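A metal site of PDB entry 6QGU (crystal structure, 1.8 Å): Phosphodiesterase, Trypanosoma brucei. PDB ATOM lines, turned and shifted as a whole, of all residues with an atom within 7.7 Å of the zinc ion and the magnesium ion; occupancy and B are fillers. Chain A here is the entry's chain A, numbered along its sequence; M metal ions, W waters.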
ATOM      1  N   TYR A 105      -5.698 -17.532  14.108  1.00  0.00           N
ATOM      2  CA  TYR A 105      -5.844 -16.060  14.033  1.00  0.00           C
ATOM      3  C   TYR A 105      -6.969 -15.622  14.968  1.00  0.00           C
ATOM      4  O   TYR A 105      -7.918 -16.383  15.177  1.00  0.00           O
ATOM      5  CB  TYR A 105      -6.025 -15.581  12.595  1.00  0.00           C
ATOM      6  CG  TYR A 105      -4.694 -15.707  11.896  1.00  0.00           C
ATOM      7  CD1 TYR A 105      -3.715 -14.744  12.075  1.00  0.00           C
ATOM      8  CD2 TYR A 105      -4.380 -16.856  11.178  1.00  0.00           C
ATOM      9  CE1 TYR A 105      -2.460 -14.896  11.505  1.00  0.00           C
ATOM     10  CE2 TYR A 105      -3.136 -17.011  10.579  1.00  0.00           C
ATOM     11  CZ  TYR A 105      -2.178 -16.030  10.765  1.00  0.00           C
ATOM     12  OH  TYR A 105      -0.940 -16.193  10.234  1.00  0.00           O
ATOM     13  N   TYR A 110      -6.818  -5.799  12.571  1.00  0.00           N
ATOM     14  CA  TYR A 110      -5.853  -5.813  11.442  1.00  0.00           C
ATOM     15  C   TYR A 110      -5.120  -7.159  11.346  1.00  0.00           C
ATOM     16  O   TYR A 110      -5.207  -7.744  10.253  1.00  0.00           O
ATOM     17  CB  TYR A 110      -4.858  -4.668  11.555  1.00  0.00           C
ATOM     18  CG  TYR A 110      -3.902  -4.634  10.392  1.00  0.00           C
ATOM     19  CD1 TYR A 110      -4.305  -4.137   9.166  1.00  0.00           C
ATOM     20  CD2 TYR A 110      -2.608  -5.126  10.505  1.00  0.00           C
ATOM     21  CE1 TYR A 110      -3.448  -4.093   8.083  1.00  0.00           C
ATOM     22  CE2 TYR A 110      -1.749  -5.123   9.415  1.00  0.00           C
ATOM     23  CZ  TYR A 110      -2.183  -4.629   8.190  1.00  0.00           C
ATOM     24  OH  TYR A 110      -1.382  -4.564   7.084  1.00  0.00           O
ATOM     25  N   HIS A 111      -4.452  -7.627  12.404  1.00  0.00           N
ATOM     26  CA  HIS A 111      -3.608  -8.855  12.351  1.00  0.00           C
ATOM     27  C   HIS A 111      -4.473 -10.090  12.541  1.00  0.00           C
ATOM     28  O   HIS A 111      -4.243 -10.888  13.454  1.00  0.00           O
ATOM     29  CB  HIS A 111      -2.477  -8.786  13.353  1.00  0.00           C
ATOM     30  CG  HIS A 111      -1.434  -7.786  12.989  1.00  0.00           C
ATOM     31  ND1 HIS A 111      -1.327  -6.572  13.616  1.00  0.00           N
ATOM     32  CD2 HIS A 111      -0.445  -7.847  12.102  1.00  0.00           C
ATOM     33  CE1 HIS A 111      -0.301  -5.904  13.107  1.00  0.00           C
ATOM     34  NE2 HIS A 111       0.256  -6.675  12.163  1.00  0.00           N
ATOM     35  N   ASN A 112      -5.392 -10.278  11.630  1.00  0.00           N
ATOM     36  CA  ASN A 112      -6.359 -11.404  11.623  1.00  0.00           C
ATOM     37  C   ASN A 112      -6.086 -12.238  10.375  1.00  0.00           C
ATOM     38  O   ASN A 112      -5.145 -11.926   9.621  1.00  0.00           O
ATOM     39  CB  ASN A 112      -7.749 -10.805  11.740  1.00  0.00           C
ATOM     40  CG  ASN A 112      -8.051  -9.803  10.653  1.00  0.00           C
ATOM     41  OD1 ASN A 112      -7.757 -10.044   9.479  1.00  0.00           O
ATOM     42  ND2 ASN A 112      -8.621  -8.673  11.041  1.00  0.00           N
ATOM     43  N   HIS A 115      -5.587 -10.404   6.936  1.00  0.00           N
ATOM     44  CA  HIS A 115      -4.235  -9.841   6.700  1.00  0.00           C
ATOM     45  C   HIS A 115      -3.329 -10.885   6.036  1.00  0.00           C
ATOM     46  O   HIS A 115      -2.623 -10.534   5.078  1.00  0.00           O
ATOM     47  CB  HIS A 115      -3.640  -9.279   7.977  1.00  0.00           C
ATOM     48  CG  HIS A 115      -2.185  -8.960   7.844  1.00  0.00           C
ATOM     49  ND1 HIS A 115      -1.698  -7.988   6.995  1.00  0.00           N
ATOM     50  CD2 HIS A 115      -1.121  -9.491   8.488  1.00  0.00           C
ATOM     51  CE1 HIS A 115      -0.365  -7.948   7.096  1.00  0.00           C
ATOM     52  NE2 HIS A 115       0.028  -8.854   8.033  1.00  0.00           N
ATOM     53  N   VAL A 116      -3.308 -12.104   6.532  1.00  0.00           N
ATOM     54  CA  VAL A 116      -2.318 -13.118   6.037  1.00  0.00           C
ATOM     55  C   VAL A 116      -2.771 -13.624   4.668  1.00  0.00           C
ATOM     56  O   VAL A 116      -1.930 -13.857   3.790  1.00  0.00           O
ATOM     57  CB  VAL A 116      -2.031 -14.206   7.085  1.00  0.00           C
ATOM     58  CG1 VAL A 116      -1.579 -13.582   8.379  1.00  0.00           C
ATOM     59  CG2 VAL A 116      -3.187 -15.154   7.369  1.00  0.00           C
ATOM     60  N   VAL A 119      -1.717 -10.957   2.378  1.00  0.00           N
ATOM     61  CA  VAL A 119      -0.236 -10.993   2.118  1.00  0.00           C
ATOM     62  C   VAL A 119       0.083 -12.123   1.117  1.00  0.00           C
ATOM     63  O   VAL A 119       0.899 -11.906   0.205  1.00  0.00           O
ATOM     64  CB  VAL A 119       0.533 -11.102   3.436  1.00  0.00           C
ATOM     65  CG1 VAL A 119       1.991 -11.483   3.229  1.00  0.00           C
ATOM     66  CG2 VAL A 119       0.422  -9.829   4.270  1.00  0.00           C
ATOM     67  N   ALA A 148       3.362 -16.837   3.994  1.00  0.00           N
ATOM     68  CA  ALA A 148       2.396 -15.733   4.138  1.00  0.00           C
ATOM     69  C   ALA A 148       1.309 -16.105   5.136  1.00  0.00           C
ATOM     70  O   ALA A 148       0.939 -15.273   5.970  1.00  0.00           O
ATOM     71  CB  ALA A 148       1.809 -15.397   2.804  1.00  0.00           C
ATOM     72  N   HIS A 151       2.580 -16.167   8.987  1.00  0.00           N
ATOM     73  CA  HIS A 151       3.602 -15.178   9.395  1.00  0.00           C
ATOM     74  C   HIS A 151       3.143 -14.333  10.584  1.00  0.00           C
ATOM     75  O   HIS A 151       3.991 -13.704  11.179  1.00  0.00           O
ATOM     76  CB  HIS A 151       4.063 -14.345   8.215  1.00  0.00           C
ATOM     77  CG  HIS A 151       3.256 -13.134   7.998  1.00  0.00           C
ATOM     78  ND1 HIS A 151       2.139 -13.142   7.189  1.00  0.00           N
ATOM     79  CD2 HIS A 151       3.342 -11.896   8.524  1.00  0.00           C
ATOM     80  CE1 HIS A 151       1.613 -11.922   7.197  1.00  0.00           C
ATOM     81  NE2 HIS A 151       2.330 -11.171   7.991  1.00  0.00           N
ATOM     82  N   ASP A 152       1.861 -14.355  10.946  1.00  0.00           N
ATOM     83  CA  ASP A 152       1.347 -13.589  12.110  1.00  0.00           C
ATOM     84  C   ASP A 152       0.508 -14.466  13.030  1.00  0.00           C
ATOM     85  O   ASP A 152      -0.337 -13.909  13.696  1.00  0.00           O
ATOM     86  CB  ASP A 152       0.516 -12.403  11.604  1.00  0.00           C
ATOM     87  CG  ASP A 152       1.350 -11.179  11.276  1.00  0.00           C
ATOM     88  OD1 ASP A 152       2.398 -10.964  11.920  1.00  0.00           O
ATOM     89  OD2 ASP A 152       0.912 -10.439  10.394  1.00  0.00           O
ATOM     90  N   LEU A 153       0.753 -15.784  13.074  1.00  0.00           N
ATOM     91  CA  LEU A 153      -0.102 -16.719  13.854  1.00  0.00           C
ATOM     92  C   LEU A 153      -0.252 -16.234  15.304  1.00  0.00           C
ATOM     93  O   LEU A 153       0.738 -15.955  15.986  1.00  0.00           O
ATOM     94  CB  LEU A 153       0.509 -18.129  13.864  1.00  0.00           C
ATOM     95  CG  LEU A 153       0.390 -18.889  12.554  1.00  0.00           C
ATOM     96  CD1 LEU A 153       1.312 -20.073  12.574  1.00  0.00           C
ATOM     97  CD2 LEU A 153      -1.072 -19.288  12.257  1.00  0.00           C
ATOM     98  N   HIS A 155      -1.389 -13.558  16.609  1.00  0.00           N
ATOM     99  CA  HIS A 155      -1.220 -12.117  16.911  1.00  0.00           C
ATOM    100  C   HIS A 155      -2.392 -11.648  17.764  1.00  0.00           C
ATOM    101  O   HIS A 155      -3.539 -11.956  17.392  1.00  0.00           O
ATOM    102  CB  HIS A 155      -1.161 -11.284  15.616  1.00  0.00           C
ATOM    103  CG  HIS A 155      -0.405 -10.029  15.788  1.00  0.00           C
ATOM    104  ND1 HIS A 155      -0.887  -8.982  16.569  1.00  0.00           N
ATOM    105  CD2 HIS A 155       0.749  -9.609  15.222  1.00  0.00           C
ATOM    106  CE1 HIS A 155      -0.003  -7.991  16.514  1.00  0.00           C
ATOM    107  NE2 HIS A 155       1.003  -8.361  15.683  1.00  0.00           N
ATOM    108  N   ASN A 160       5.611  -5.795  19.494  1.00  0.00           N
ATOM    109  CA  ASN A 160       6.707  -6.312  20.361  1.00  0.00           C
ATOM    110  C   ASN A 160       6.910  -5.354  21.535  1.00  0.00           C
ATOM    111  O   ASN A 160       7.089  -5.796  22.680  1.00  0.00           O
ATOM    112  CB  ASN A 160       7.992  -6.530  19.571  1.00  0.00           C
ATOM    113  CG  ASN A 160       7.850  -7.702  18.620  1.00  0.00           C
ATOM    114  OD1 ASN A 160       6.925  -8.523  18.761  1.00  0.00           O
ATOM    115  ND2 ASN A 160       8.717  -7.755  17.618  1.00  0.00           N
ATOM    116  N   LEU A 183       7.013 -11.433  18.953  1.00  0.00           N
ATOM    117  CA  LEU A 183       5.892 -12.035  18.223  1.00  0.00           C
ATOM    118  C   LEU A 183       6.415 -12.979  17.137  1.00  0.00           C
ATOM    119  O   LEU A 183       5.817 -14.040  16.962  1.00  0.00           O
ATOM    120  CB  LEU A 183       4.988 -10.954  17.637  1.00  0.00           C
ATOM    121  CG  LEU A 183       4.103 -10.275  18.682  1.00  0.00           C
ATOM    122  CD1 LEU A 183       3.388  -9.119  18.049  1.00  0.00           C
ATOM    123  CD2 LEU A 183       3.111 -11.247  19.293  1.00  0.00           C
ATOM    124  N   GLU A 184       7.470 -12.599  16.420  1.00  0.00           N
ATOM    125  CA  GLU A 184       7.915 -13.345  15.226  1.00  0.00           C
ATOM    126  C   GLU A 184       8.381 -14.727  15.675  1.00  0.00           C
ATOM    127  O   GLU A 184       8.057 -15.730  15.003  1.00  0.00           O
ATOM    128  CB  GLU A 184       8.988 -12.551  14.462  1.00  0.00           C
ATOM    129  CG  GLU A 184       8.398 -11.265  13.832  1.00  0.00           C
ATOM    130  CD  GLU A 184       8.110 -10.084  14.763  1.00  0.00           C
ATOM    131  OE1 GLU A 184       8.617 -10.064  15.922  1.00  0.00           O
ATOM    132  OE2 GLU A 184       7.321  -9.191  14.355  1.00  0.00           O
ATOM    133  N   HIS A 187       5.156 -16.706  16.341  1.00  0.00           N
ATOM    134  CA  HIS A 187       4.527 -17.171  15.089  1.00  0.00           C
ATOM    135  C   HIS A 187       5.272 -18.402  14.591  1.00  0.00           C
ATOM    136  O   HIS A 187       4.595 -19.325  14.120  1.00  0.00           O
ATOM    137  CB  HIS A 187       4.491 -16.091  13.989  1.00  0.00           C
ATOM    138  CG  HIS A 187       4.027 -14.743  14.413  1.00  0.00           C
ATOM    139  ND1 HIS A 187       2.896 -14.524  15.209  1.00  0.00           N
ATOM    140  CD2 HIS A 187       4.551 -13.519  14.149  1.00  0.00           C
ATOM    141  CE1 HIS A 187       2.750 -13.224  15.355  1.00  0.00           C
ATOM    142  NE2 HIS A 187       3.736 -12.598  14.704  1.00  0.00           N
ATOM    143  N   VAL A 222       9.813 -15.223   8.344  1.00  0.00           N
ATOM    144  CA  VAL A 222       8.951 -14.731   9.442  1.00  0.00           C
ATOM    145  C   VAL A 222       9.777 -13.817  10.372  1.00  0.00           C
ATOM    146  O   VAL A 222       9.296 -12.727  10.730  1.00  0.00           O
ATOM    147  CB  VAL A 222       8.261 -15.877  10.191  1.00  0.00           C
ATOM    148  CG1 VAL A 222       7.523 -15.352  11.421  1.00  0.00           C
ATOM    149  CG2 VAL A 222       7.359 -16.648   9.276  1.00  0.00           C
ATOM    150  N   THR A 225      10.266 -10.238   9.273  1.00  0.00           N
ATOM    151  CA  THR A 225       9.118  -9.297   9.287  1.00  0.00           C
ATOM    152  C   THR A 225       9.188  -8.347  10.480  1.00  0.00           C
ATOM    153  O   THR A 225       8.364  -7.409  10.521  1.00  0.00           O
ATOM    154  CB  THR A 225       7.742  -9.985   9.286  1.00  0.00           C
ATOM    155  OG1 THR A 225       7.600 -10.835  10.421  1.00  0.00           O
ATOM    156  CG2 THR A 225       7.480 -10.752   8.020  1.00  0.00           C
ATOM    157  N   ASP A 226      10.073  -8.565  11.453  1.00  0.00           N
ATOM    158  CA  ASP A 226      10.208  -7.619  12.589  1.00  0.00           C
ATOM    159  C   ASP A 226      10.704  -6.269  12.045  1.00  0.00           C
ATOM    160  O   ASP A 226      11.846  -6.200  11.561  1.00  0.00           O
ATOM    161  CB  ASP A 226      11.182  -8.155  13.634  1.00  0.00           C
ATOM    162  CG  ASP A 226      11.346  -7.291  14.875  1.00  0.00           C
ATOM    163  OD1 ASP A 226      10.808  -6.162  14.907  1.00  0.00           O
ATOM    164  OD2 ASP A 226      12.049  -7.760  15.802  1.00  0.00           O
ATOM    165  N   MET A 227       9.894  -5.225  12.157  1.00  0.00           N
ATOM    166  CA  MET A 227      10.202  -3.893  11.568  1.00  0.00           C
ATOM    167  C   MET A 227      11.429  -3.259  12.221  1.00  0.00           C
ATOM    168  O   MET A 227      12.037  -2.382  11.594  1.00  0.00           O
ATOM    169  CB  MET A 227       8.984  -2.970  11.621  1.00  0.00           C
ATOM    170  CG  MET A 227       7.977  -3.248  10.538  1.00  0.00           C
ATOM    171  SD  MET A 227       8.644  -3.208   8.808  1.00  0.00           S
ATOM    172  CE  MET A 227       8.662  -1.438   8.556  1.00  0.00           C
ATOM    173  N   LEU A 260       8.473 -11.289   1.429  1.00  0.00           N
ATOM    174  CA  LEU A 260       7.526 -11.333   2.557  1.00  0.00           C
ATOM    175  C   LEU A 260       7.416  -9.965   3.230  1.00  0.00           C
ATOM    176  O   LEU A 260       6.325  -9.539   3.530  1.00  0.00           O
ATOM    177  CB  LEU A 260       7.920 -12.396   3.584  1.00  0.00           C
ATOM    178  CG  LEU A 260       6.960 -12.510   4.766  1.00  0.00           C
ATOM    179  CD1 LEU A 260       5.542 -12.778   4.322  1.00  0.00           C
ATOM    180  CD2 LEU A 260       7.390 -13.613   5.707  1.00  0.00           C
ATOM    181  N   GLY A 263       5.213  -7.835   0.932  1.00  0.00           N
ATOM    182  CA  GLY A 263       3.801  -8.217   1.098  1.00  0.00           C
ATOM    183  C   GLY A 263       3.238  -7.625   2.384  1.00  0.00           C
ATOM    184  O   GLY A 263       2.084  -7.098   2.419  1.00  0.00           O
ATOM    185  N   ASP A 264       4.012  -7.703   3.450  1.00  0.00           N
ATOM    186  CA  ASP A 264       3.583  -7.212   4.770  1.00  0.00           C
ATOM    187  C   ASP A 264       3.360  -5.687   4.762  1.00  0.00           C
ATOM    188  O   ASP A 264       2.543  -5.233   5.524  1.00  0.00           O
ATOM    189  CB  ASP A 264       4.571  -7.686   5.814  1.00  0.00           C
ATOM    190  CG  ASP A 264       3.969  -7.894   7.192  1.00  0.00           C
ATOM    191  OD1 ASP A 264       2.769  -8.200   7.259  1.00  0.00           O
ATOM    192  OD2 ASP A 264       4.743  -7.814   8.168  1.00  0.00           O
ATOM    193  N   ILE A 265       4.101  -4.867   4.015  1.00  0.00           N
ATOM    194  CA  ILE A 265       3.870  -3.405   3.995  1.00  0.00           C
ATOM    195  C   ILE A 265       3.282  -2.959   2.639  1.00  0.00           C
ATOM    196  O   ILE A 265       3.492  -1.794   2.244  1.00  0.00           O
ATOM    197  CB  ILE A 265       5.162  -2.672   4.378  1.00  0.00           C
ATOM    198  CG1 ILE A 265       6.279  -2.952   3.388  1.00  0.00           C
ATOM    199  CG2 ILE A 265       5.591  -3.006   5.804  1.00  0.00           C
ATOM    200  CD1 ILE A 265       7.419  -1.959   3.492  1.00  0.00           C
HETATM  201 ZN    ZN M   1       1.908  -9.210   8.909  1.00  0.00          ZN
HETATM  202 MG    MG M   2       3.957  -9.651  12.006  1.00  0.00          MG
HETATM  203  O   HOH W   1       1.752  -7.198   9.914  1.00  0.00           O
HETATM  204  O   HOH W   2       3.636  -9.149  10.135  1.00  0.00           O
HETATM  205  O   HOH W   3       4.203 -10.161  14.153  1.00  0.00           O
HETATM  206  O   HOH W   4       5.289 -11.587  11.760  1.00  0.00           O
HETATM  207  O   HOH W   5       5.961  -8.590  12.044  1.00  0.00           O
HETATM  208  O   HOH W   6       2.992  -7.821  12.821  1.00  0.00           O
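Of the 24 residues printed, 1 comes within 4 Å of the magnesium ion.
The zinc ion is bound by NE2 of His 115, at 2.1 Å. OD1 of Asp 264 is bound to the zinc ion (2.1 Å). Water W2 binds the zinc ion (2.1 Å). OD2 of Asp 152 is bound to the zinc ion, 2.2 Å away. NE2 of His 151 binds the zinc ion. The zinc ion is bound by water W1.
Water W4 lies within hydrogen-bond range of the backbone carbonyl oxygen (O) of His 151, the side-chain hydroxyl (OG1) of Thr 225 and a ring nitrogen (NE2) of His 187. Water W3 lies within hydrogen-bond range of a ring nitrogen (NE2) of His 187 (2.5 Å) and the side-chain carboxylate of Glu 184 (3.3 Å). Water W5 bridges OE2 of Glu 184 (2.7 Å) and O of Thr 225 (3.1 Å).
The side-chain carboxylate of Asp 152 sits close to a ring nitrogen (NE2) of His 187. A ring nitrogen (ND1) of His 151 sits at hydrogen-bond distance from the backbone carbonyl oxygen (O) of Ala 148. N of His 115 is in hydrogen-bond range of OD1 of Asn 112 (3.4 Å). A ring nitrogen (ND1) of His 115 sits at hydrogen-bond distance from the side-chain hydroxyl (OH) of Tyr 110. N of Asp 152 sits at hydrogen-bond distance from OH of Tyr 105.
Of the 24 residues printed, 4 come within 4 Å of the zinc ion.
The magnesium ion is bound by water W2 (2.0 Å). The magnesium ion is bound by OD1 of Asp 152. The magnesium ion is bound by water W3 (2.2 Å). Water W6 is bound to the magnesium ion (2.2 Å). The magnesium ion is bound by water W5. Water W4 is bound to the magnesium ion.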
